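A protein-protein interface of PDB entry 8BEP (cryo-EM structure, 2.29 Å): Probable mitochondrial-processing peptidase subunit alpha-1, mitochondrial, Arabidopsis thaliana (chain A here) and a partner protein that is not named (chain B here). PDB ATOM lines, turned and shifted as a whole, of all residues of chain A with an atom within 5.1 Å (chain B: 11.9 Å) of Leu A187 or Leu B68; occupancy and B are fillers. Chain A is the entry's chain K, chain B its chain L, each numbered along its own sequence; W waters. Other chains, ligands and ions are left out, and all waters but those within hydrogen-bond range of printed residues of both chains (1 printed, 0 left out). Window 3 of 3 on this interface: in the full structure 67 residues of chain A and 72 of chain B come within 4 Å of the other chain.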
ATOM      1  N   SER A 130      -5.058  -0.261  10.474  1.00  0.00           N
ATOM      2  CA  SER A 130      -5.432  -1.325   9.549  1.00  0.00           C
ATOM      3  C   SER A 130      -5.361  -2.691  10.224  1.00  0.00           C
ATOM      4  O   SER A 130      -4.461  -2.965  11.019  1.00  0.00           O
ATOM      5  CB  SER A 130      -4.518  -1.313   8.322  1.00  0.00           C
ATOM      6  OG  SER A 130      -4.483  -0.046   7.698  1.00  0.00           O
ATOM      7  N   THR A 131      -6.324  -3.546   9.905  1.00  0.00           N
ATOM      8  CA  THR A 131      -6.328  -4.938  10.327  1.00  0.00           C
ATOM      9  C   THR A 131      -6.140  -5.836   9.109  1.00  0.00           C
ATOM     10  O   THR A 131      -6.045  -5.374   7.969  1.00  0.00           O
ATOM     11  CB  THR A 131      -7.621  -5.299  11.067  1.00  0.00           C
ATOM     12  OG1 THR A 131      -8.713  -5.358  10.142  1.00  0.00           O
ATOM     13  CG2 THR A 131      -7.930  -4.280  12.153  1.00  0.00           C
ATOM     14  N   LEU A 132      -6.095  -7.143   9.361  1.00  0.00           N
ATOM     15  CA  LEU A 132      -6.004  -8.107   8.272  1.00  0.00           C
ATOM     16  C   LEU A 132      -7.286  -8.174   7.452  1.00  0.00           C
ATOM     17  O   LEU A 132      -7.273  -8.735   6.355  1.00  0.00           O
ATOM     18  CB  LEU A 132      -5.659  -9.492   8.825  1.00  0.00           C
ATOM     19  CG  LEU A 132      -4.406  -9.579   9.701  1.00  0.00           C
ATOM     20  CD1 LEU A 132      -4.272 -10.959  10.323  1.00  0.00           C
ATOM     21  CD2 LEU A 132      -3.154  -9.219   8.911  1.00  0.00           C
ATOM     22  N   ALA A 185      -2.710  -5.410  11.510  1.00  0.00           N
ATOM     23  CA  ALA A 185      -1.824  -5.682  10.390  1.00  0.00           C
ATOM     24  C   ALA A 185      -0.400  -5.223  10.671  1.00  0.00           C
ATOM     25  O   ALA A 185       0.549  -5.819  10.152  1.00  0.00           O
ATOM     26  CB  ALA A 185      -2.364  -5.017   9.124  1.00  0.00           C
ATOM     27  N   PHE A 186      -0.237  -4.189  11.497  1.00  0.00           N
ATOM     28  CA  PHE A 186       1.064  -3.596  11.808  1.00  0.00           C
ATOM     29  C   PHE A 186       1.876  -3.330  10.541  1.00  0.00           C
ATOM     30  O   PHE A 186       3.043  -3.705  10.427  1.00  0.00           O
ATOM     31  CB  PHE A 186       1.846  -4.464  12.796  1.00  0.00           C
ATOM     32  CG  PHE A 186       1.245  -4.503  14.170  1.00  0.00           C
ATOM     33  CD1 PHE A 186       0.836  -3.335  14.795  1.00  0.00           C
ATOM     34  CD2 PHE A 186       1.085  -5.702  14.836  1.00  0.00           C
ATOM     35  CE1 PHE A 186       0.278  -3.366  16.055  1.00  0.00           C
ATOM     36  CE2 PHE A 186       0.529  -5.741  16.100  1.00  0.00           C
ATOM     37  CZ  PHE A 186       0.123  -4.572  16.710  1.00  0.00           C
ATOM     38  N   LEU A 187       1.236  -2.669   9.577  1.00  0.00           N
ATOM     39  CA  LEU A 187       1.913  -2.304   8.341  1.00  0.00           C
ATOM     40  C   LEU A 187       3.039  -1.321   8.627  1.00  0.00           C
ATOM     41  O   LEU A 187       2.916  -0.439   9.482  1.00  0.00           O
ATOM     42  CB  LEU A 187       0.920  -1.698   7.349  1.00  0.00           C
ATOM     43  CG  LEU A 187      -0.382  -2.462   7.120  1.00  0.00           C
ATOM     44  CD1 LEU A 187      -1.335  -1.647   6.262  1.00  0.00           C
ATOM     45  CD2 LEU A 187      -0.114  -3.831   6.500  1.00  0.00           C
ATOM     46  N   ASP A 188       4.143  -1.471   7.892  1.00  0.00           N
ATOM     47  CA  ASP A 188       5.360  -0.734   8.218  1.00  0.00           C
ATOM     48  C   ASP A 188       5.184   0.771   8.050  1.00  0.00           C
ATOM     49  O   ASP A 188       5.708   1.550   8.850  1.00  0.00           O
ATOM     50  CB  ASP A 188       6.521  -1.238   7.367  1.00  0.00           C
ATOM     51  CG  ASP A 188       7.019  -2.590   7.815  1.00  0.00           C
ATOM     52  OD1 ASP A 188       7.283  -2.754   9.025  1.00  0.00           O
ATOM     53  OD2 ASP A 188       7.142  -3.495   6.962  1.00  0.00           O
ATOM     54  N   TRP A 189       4.470   1.207   7.008  1.00  0.00           N
ATOM     55  CA  TRP A 189       4.304   2.645   6.806  1.00  0.00           C
ATOM     56  C   TRP A 189       3.449   3.268   7.909  1.00  0.00           C
ATOM     57  O   TRP A 189       3.747   4.371   8.386  1.00  0.00           O
ATOM     58  CB  TRP A 189       3.720   2.937   5.417  1.00  0.00           C
ATOM     59  CG  TRP A 189       2.627   2.017   4.941  1.00  0.00           C
ATOM     60  CD1 TRP A 189       1.291   2.283   4.916  1.00  0.00           C
ATOM     61  CD2 TRP A 189       2.781   0.704   4.382  1.00  0.00           C
ATOM     62  NE1 TRP A 189       0.602   1.216   4.397  1.00  0.00           N
ATOM     63  CE2 TRP A 189       1.493   0.233   4.060  1.00  0.00           C
ATOM     64  CE3 TRP A 189       3.881  -0.122   4.131  1.00  0.00           C
ATOM     65  CZ2 TRP A 189       1.274  -1.023   3.500  1.00  0.00           C
ATOM     66  CZ3 TRP A 189       3.660  -1.370   3.576  1.00  0.00           C
ATOM     67  CH2 TRP A 189       2.368  -1.808   3.267  1.00  0.00           C
ATOM     68  N   GLU A 190       2.404   2.564   8.347  1.00  0.00           N
ATOM     69  CA  GLU A 190       1.580   3.054   9.449  1.00  0.00           C
ATOM     70  C   GLU A 190       2.382   3.123  10.748  1.00  0.00           C
ATOM     71  O   GLU A 190       2.286   4.099  11.506  1.00  0.00           O
ATOM     72  CB  GLU A 190       0.347   2.158   9.604  1.00  0.00           C
ATOM     73  CG  GLU A 190      -0.581   2.197   8.391  1.00  0.00           C
ATOM     74  CD  GLU A 190      -1.921   1.514   8.618  1.00  0.00           C
ATOM     75  OE1 GLU A 190      -2.139   0.942   9.703  1.00  0.00           O
ATOM     76  OE2 GLU A 190      -2.759   1.536   7.695  1.00  0.00           O
ATOM     77  N   VAL A 191       3.196   2.096  11.010  1.00  0.00           N
ATOM     78  CA  VAL A 191       4.042   2.089  12.202  1.00  0.00           C
ATOM     79  C   VAL A 191       5.046   3.236  12.154  1.00  0.00           C
ATOM     80  O   VAL A 191       5.297   3.902  13.163  1.00  0.00           O
ATOM     81  CB  VAL A 191       4.744   0.728  12.361  1.00  0.00           C
ATOM     82  CG1 VAL A 191       5.710   0.762  13.532  1.00  0.00           C
ATOM     83  CG2 VAL A 191       3.724  -0.370  12.576  1.00  0.00           C
ATOM     84  N   ASN A 192       5.644   3.475  10.986  1.00  0.00           N
ATOM     85  CA  ASN A 192       6.609   4.565  10.861  1.00  0.00           C
ATOM     86  C   ASN A 192       5.945   5.918  11.090  1.00  0.00           C
ATOM     87  O   ASN A 192       6.530   6.807  11.722  1.00  0.00           O
ATOM     88  CB  ASN A 192       7.283   4.521   9.490  1.00  0.00           C
ATOM     89  CG  ASN A 192       8.214   3.335   9.333  1.00  0.00           C
ATOM     90  OD1 ASN A 192       8.552   2.662  10.305  1.00  0.00           O
ATOM     91  ND2 ASN A 192       8.637   3.076   8.103  1.00  0.00           N
ATOM     92  N   GLU B  59      10.680 -10.944  -0.471  1.00  0.00           N
ATOM     93  CA  GLU B  59       9.808 -12.086  -0.215  1.00  0.00           C
ATOM     94  C   GLU B  59       8.970 -11.873   1.040  1.00  0.00           C
ATOM     95  O   GLU B  59       7.773 -12.186   1.057  1.00  0.00           O
ATOM     96  CB  GLU B  59      10.636 -13.365  -0.098  1.00  0.00           C
ATOM     97  CG  GLU B  59      11.214 -13.851  -1.412  1.00  0.00           C
ATOM     98  CD  GLU B  59      10.160 -14.038  -2.487  1.00  0.00           C
ATOM     99  OE1 GLU B  59       9.018 -14.412  -2.154  1.00  0.00           O
ATOM    100  OE2 GLU B  59      10.475 -13.811  -3.672  1.00  0.00           O
ATOM    101  N   ILE B  60       9.580 -11.331   2.096  1.00  0.00           N
ATOM    102  CA  ILE B  60       8.843 -11.084   3.335  1.00  0.00           C
ATOM    103  C   ILE B  60       7.696 -10.110   3.089  1.00  0.00           C
ATOM    104  O   ILE B  60       6.545 -10.360   3.480  1.00  0.00           O
ATOM    105  CB  ILE B  60       9.790 -10.566   4.432  1.00  0.00           C
ATOM    106  CG1 ILE B  60      10.567 -11.713   5.068  1.00  0.00           C
ATOM    107  CG2 ILE B  60       9.020  -9.812   5.502  1.00  0.00           C
ATOM    108  CD1 ILE B  60      11.789 -11.242   5.791  1.00  0.00           C
ATOM    109  N   ILE B  61       7.988  -8.986   2.427  1.00  0.00           N
ATOM    110  CA  ILE B  61       6.934  -7.998   2.202  1.00  0.00           C
ATOM    111  C   ILE B  61       5.865  -8.549   1.258  1.00  0.00           C
ATOM    112  O   ILE B  61       4.678  -8.245   1.416  1.00  0.00           O
ATOM    113  CB  ILE B  61       7.526  -6.659   1.708  1.00  0.00           C
ATOM    114  CG1 ILE B  61       6.505  -5.527   1.855  1.00  0.00           C
ATOM    115  CG2 ILE B  61       7.998  -6.742   0.269  1.00  0.00           C
ATOM    116  CD1 ILE B  61       5.859  -5.439   3.216  1.00  0.00           C
ATOM    117  N   LYS B  62       6.253  -9.380   0.283  1.00  0.00           N
ATOM    118  CA  LYS B  62       5.272  -9.974  -0.620  1.00  0.00           C
ATOM    119  C   LYS B  62       4.326 -10.913   0.124  1.00  0.00           C
ATOM    120  O   LYS B  62       3.113 -10.894  -0.112  1.00  0.00           O
ATOM    121  CB  LYS B  62       5.983 -10.713  -1.753  1.00  0.00           C
ATOM    122  CG  LYS B  62       6.406  -9.827  -2.914  1.00  0.00           C
ATOM    123  CD  LYS B  62       6.876 -10.656  -4.100  1.00  0.00           C
ATOM    124  CE  LYS B  62       8.261 -11.227  -3.868  1.00  0.00           C
ATOM    125  NZ  LYS B  62       8.816 -11.859  -5.093  1.00  0.00           N
ATOM    126  N   ASN B  63       4.859 -11.740   1.026  1.00  0.00           N
ATOM    127  CA  ASN B  63       3.997 -12.615   1.818  1.00  0.00           C
ATOM    128  C   ASN B  63       3.061 -11.807   2.711  1.00  0.00           C
ATOM    129  O   ASN B  63       1.867 -12.122   2.831  1.00  0.00           O
ATOM    130  CB  ASN B  63       4.845 -13.573   2.653  1.00  0.00           C
ATOM    131  CG  ASN B  63       5.642 -14.530   1.800  1.00  0.00           C
ATOM    132  OD1 ASN B  63       5.141 -15.057   0.809  1.00  0.00           O
ATOM    133  ND2 ASN B  63       6.894 -14.754   2.175  1.00  0.00           N
ATOM    134  N   LYS B  64       3.582 -10.743   3.327  1.00  0.00           N
ATOM    135  CA  LYS B  64       2.726  -9.886   4.143  1.00  0.00           C
ATOM    136  C   LYS B  64       1.598  -9.282   3.317  1.00  0.00           C
ATOM    137  O   LYS B  64       0.444  -9.256   3.758  1.00  0.00           O
ATOM    138  CB  LYS B  64       3.555  -8.788   4.801  1.00  0.00           C
ATOM    139  CG  LYS B  64       3.354  -8.708   6.290  1.00  0.00           C
ATOM    140  CD  LYS B  64       1.984  -8.146   6.611  1.00  0.00           C
ATOM    141  CE  LYS B  64       1.848  -7.851   8.086  1.00  0.00           C
ATOM    142  NZ  LYS B  64       0.421  -7.847   8.506  1.00  0.00           N
ATOM    143  N   ILE B  65       1.910  -8.797   2.113  1.00  0.00           N
ATOM    144  CA  ILE B  65       0.875  -8.284   1.220  1.00  0.00           C
ATOM    145  C   ILE B  65      -0.143  -9.373   0.915  1.00  0.00           C
ATOM    146  O   ILE B  65      -1.354  -9.126   0.888  1.00  0.00           O
ATOM    147  CB  ILE B  65       1.508  -7.736  -0.073  1.00  0.00           C
ATOM    148  CG1 ILE B  65       2.104  -6.350   0.151  1.00  0.00           C
ATOM    149  CG2 ILE B  65       0.487  -7.680  -1.197  1.00  0.00           C
ATOM    150  CD1 ILE B  65       2.987  -5.917  -0.983  1.00  0.00           C
ATOM    151  N   LYS B  66       0.337 -10.597   0.687  1.00  0.00           N
ATOM    152  CA  LYS B  66      -0.553 -11.693   0.324  1.00  0.00           C
ATOM    153  C   LYS B  66      -1.573 -11.958   1.421  1.00  0.00           C
ATOM    154  O   LYS B  66      -2.748 -12.211   1.132  1.00  0.00           O
ATOM    155  CB  LYS B  66       0.272 -12.947   0.002  1.00  0.00           C
ATOM    156  CG  LYS B  66       1.163 -12.906  -1.253  1.00  0.00           C
ATOM    157  CD  LYS B  66       1.977 -14.180  -1.503  1.00  0.00           C
ATOM    158  CE  LYS B  66       2.810 -14.072  -2.769  1.00  0.00           C
ATOM    159  NZ  LYS B  66       3.628 -15.288  -3.023  1.00  0.00           N
ATOM    160  N   LYS B  67      -1.153 -11.902   2.688  1.00  0.00           N
ATOM    161  CA  LYS B  67      -2.159 -12.207   3.706  1.00  0.00           C
ATOM    162  C   LYS B  67      -3.125 -11.053   3.976  1.00  0.00           C
ATOM    163  O   LYS B  67      -3.837 -11.102   4.984  1.00  0.00           O
ATOM    164  CB  LYS B  67      -1.509 -12.642   5.020  1.00  0.00           C
ATOM    165  CG  LYS B  67      -0.549 -11.654   5.626  1.00  0.00           C
ATOM    166  CD  LYS B  67      -0.034 -12.169   6.954  1.00  0.00           C
ATOM    167  CE  LYS B  67       1.264 -12.937   6.785  1.00  0.00           C
ATOM    168  NZ  LYS B  67       2.431 -12.036   6.586  1.00  0.00           N
ATOM    169  N   LEU B  68      -3.165 -10.021   3.135  1.00  0.00           N
ATOM    170  CA  LEU B  68      -4.211  -9.009   3.202  1.00  0.00           C
ATOM    171  C   LEU B  68      -5.248  -9.167   2.100  1.00  0.00           C
ATOM    172  O   LEU B  68      -6.212  -8.398   2.058  1.00  0.00           O
ATOM    173  CB  LEU B  68      -3.607  -7.604   3.137  1.00  0.00           C
ATOM    174  CG  LEU B  68      -2.626  -7.193   4.236  1.00  0.00           C
ATOM    175  CD1 LEU B  68      -1.803  -5.994   3.788  1.00  0.00           C
ATOM    176  CD2 LEU B  68      -3.357  -6.898   5.539  1.00  0.00           C
ATOM    177  N   GLU B  69      -5.080 -10.146   1.214  1.00  0.00           N
ATOM    178  CA  GLU B  69      -5.977 -10.339   0.087  1.00  0.00           C
ATOM    179  C   GLU B  69      -7.138 -11.276   0.394  1.00  0.00           C
ATOM    180  O   GLU B  69      -8.086 -11.332  -0.395  1.00  0.00           O
ATOM    181  CB  GLU B  69      -5.194 -10.874  -1.116  1.00  0.00           C
ATOM    182  CG  GLU B  69      -4.286  -9.845  -1.768  1.00  0.00           C
ATOM    183  CD  GLU B  69      -4.882  -9.255  -3.024  1.00  0.00           C
ATOM    184  OE1 GLU B  69      -4.199  -9.269  -4.068  1.00  0.00           O
ATOM    185  OE2 GLU B  69      -6.031  -8.770  -2.969  1.00  0.00           O
ATOM    186  N   ASN B  70      -7.094 -12.003   1.507  1.00  0.00           N
ATOM    187  CA  ASN B  70      -8.160 -12.926   1.899  1.00  0.00           C
ATOM    188  C   ASN B  70      -8.608 -12.604   3.318  1.00  0.00           C
ATOM    189  O   ASN B  70      -8.148 -13.224   4.286  1.00  0.00           O
ATOM    190  CB  ASN B  70      -7.710 -14.382   1.778  1.00  0.00           C
ATOM    191  CG  ASN B  70      -6.815 -14.616   0.576  1.00  0.00           C
ATOM    192  OD1 ASN B  70      -5.683 -15.078   0.712  1.00  0.00           O
ATOM    193  ND2 ASN B  70      -7.319 -14.294  -0.608  1.00  0.00           N
ATOM    194  N   PRO B  71      -9.500 -11.630   3.480  1.00  0.00           N
ATOM    195  CA  PRO B  71     -10.037 -11.338   4.812  1.00  0.00           C
ATOM    196  C   PRO B  71     -10.970 -12.433   5.304  1.00  0.00           C
ATOM    197  O   PRO B  71     -11.630 -13.120   4.523  1.00  0.00           O
ATOM    198  CB  PRO B  71     -10.793 -10.022   4.606  1.00  0.00           C
ATOM    199  CG  PRO B  71     -11.154 -10.032   3.164  1.00  0.00           C
ATOM    200  CD  PRO B  71     -10.016 -10.702   2.460  1.00  0.00           C
ATOM    201  N   ASP B  72     -11.022 -12.581   6.626  1.00  0.00           N
ATOM    202  CA  ASP B  72     -11.949 -13.510   7.262  1.00  0.00           C
ATOM    203  C   ASP B  72     -13.324 -12.858   7.371  1.00  0.00           C
ATOM    204  O   ASP B  72     -13.482 -11.839   8.052  1.00  0.00           O
ATOM    205  CB  ASP B  72     -11.428 -13.917   8.640  1.00  0.00           C
ATOM    206  CG  ASP B  72     -12.396 -14.808   9.393  1.00  0.00           C
ATOM    207  OD1 ASP B  72     -13.256 -15.444   8.749  1.00  0.00           O
ATOM    208  OD2 ASP B  72     -12.295 -14.877  10.634  1.00  0.00           O
ATOM    209  N   LYS B  73     -14.321 -13.462   6.718  1.00  0.00           N
ATOM    210  CA  LYS B  73     -15.642 -12.848   6.618  1.00  0.00           C
ATOM    211  C   LYS B  73     -16.373 -12.826   7.956  1.00  0.00           C
ATOM    212  O   LYS B  73     -17.402 -12.153   8.081  1.00  0.00           O
ATOM    213  CB  LYS B  73     -16.477 -13.580   5.570  1.00  0.00           C
ATOM    214  CG  LYS B  73     -16.265 -13.078   4.152  1.00  0.00           C
ATOM    215  CD  LYS B  73     -17.367 -13.554   3.212  1.00  0.00           C
ATOM    216  CE  LYS B  73     -18.515 -12.554   3.102  1.00  0.00           C
ATOM    217  NZ  LYS B  73     -19.007 -12.057   4.417  1.00  0.00           N
ATOM    218  N   LEU B  76     -16.616  -9.221   8.982  1.00  0.00           N
ATOM    219  CA  LEU B  76     -17.075  -8.283   7.960  1.00  0.00           C
ATOM    220  C   LEU B  76     -18.555  -8.492   7.663  1.00  0.00           C
ATOM    221  O   LEU B  76     -18.976  -8.554   6.508  1.00  0.00           O
ATOM    222  CB  LEU B  76     -16.248  -8.422   6.680  1.00  0.00           C
ATOM    223  CG  LEU B  76     -14.785  -7.974   6.711  1.00  0.00           C
ATOM    224  CD1 LEU B  76     -14.154  -8.130   5.340  1.00  0.00           C
ATOM    225  CD2 LEU B  76     -14.659  -6.543   7.191  1.00  0.00           C
ATOM    226  N   HIS B 374      -8.693  10.029   6.934  1.00  0.00           N
ATOM    227  CA  HIS B 374      -9.719   9.126   6.443  1.00  0.00           C
ATOM    228  C   HIS B 374     -11.139   9.539   6.798  1.00  0.00           C
ATOM    229  O   HIS B 374     -12.084   8.914   6.306  1.00  0.00           O
ATOM    230  CB  HIS B 374      -9.460   7.708   6.967  1.00  0.00           C
ATOM    231  CG  HIS B 374      -8.080   7.207   6.688  1.00  0.00           C
ATOM    232  ND1 HIS B 374      -7.503   7.273   5.439  1.00  0.00           N
ATOM    233  CD2 HIS B 374      -7.155   6.644   7.499  1.00  0.00           C
ATOM    234  CE1 HIS B 374      -6.287   6.764   5.490  1.00  0.00           C
ATOM    235  NE2 HIS B 374      -6.050   6.378   6.730  1.00  0.00           N
HETATM  236  O   HOH W   1      -7.649  -7.234   4.209  1.00  0.00           O
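NZ of Lys B64 sits at hydrogen-bond distance from O of Ala A185 (2.6 Å).
O of Ser A130 lies within hydrogen-bond range of N of Ala A185 (3.0 Å).
CD2 of Leu B68 touches O of Thr A131, 3.9 Å away.
Leu A132 touches Lys B64.
Leu A132 touches Leu B68 (CA to CD2, 3.99 Å).
Leu B68 touches Leu A187 (CD1 to CD2, 3.9 Å).
Printed residues of chain B within 4 Å of Leu A187: Leu B68 (3.9 Å).
Of the printed residues of chain A, Leu B68 touches Thr A131 (3.9 Å), Leu A132 (3.99 Å) and Leu A187 (3.9 Å).
No residue of chain B comes within 4 Å of Ser A130.
No residue of chain B comes within 4 Å of Trp A189.
Glu A190 touches none of the printed residues of chain B.
Val A191 touches none of the printed residues of chain B.
Of the printed residues of chain B, Thr A131 touches Leu B68.
Of the printed residues of chain A, Lys B64 touches Leu A132 and Ala A185.
Of the printed residues of chain B, Leu A132 touches Lys B64 and Leu B68.
The nearest residue of chain B that does not touch Leu A187 is Lys B64 (4.5 Å).
The nearest printed residue of chain A that does not touch Leu B68 is Ala A185 (4.2 Å).
The nearest printed residue of chain A that does not touch Lys B64 is Leu A187 (4.5 Å).
Hydrophobic or aromatic side chains of chain B within 4 Å of the printed part of chain A: Leu B68.
Of the 11 printed residues of chain A, 4 touch a printed residue of chain B.
Hydrophobic or aromatic side chains of chain A that line the printed part of chain B: Leu A132 and Leu A187.
Among the printed residues, no Asp or Glu carboxylate lies within 4 Å of a Lys or Arg side-chain nitrogen of the other chain.
Water W1 lies within hydrogen-bond range of O of Leu A132 (2.6 Å) and O of Leu B68 (2.8 Å).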
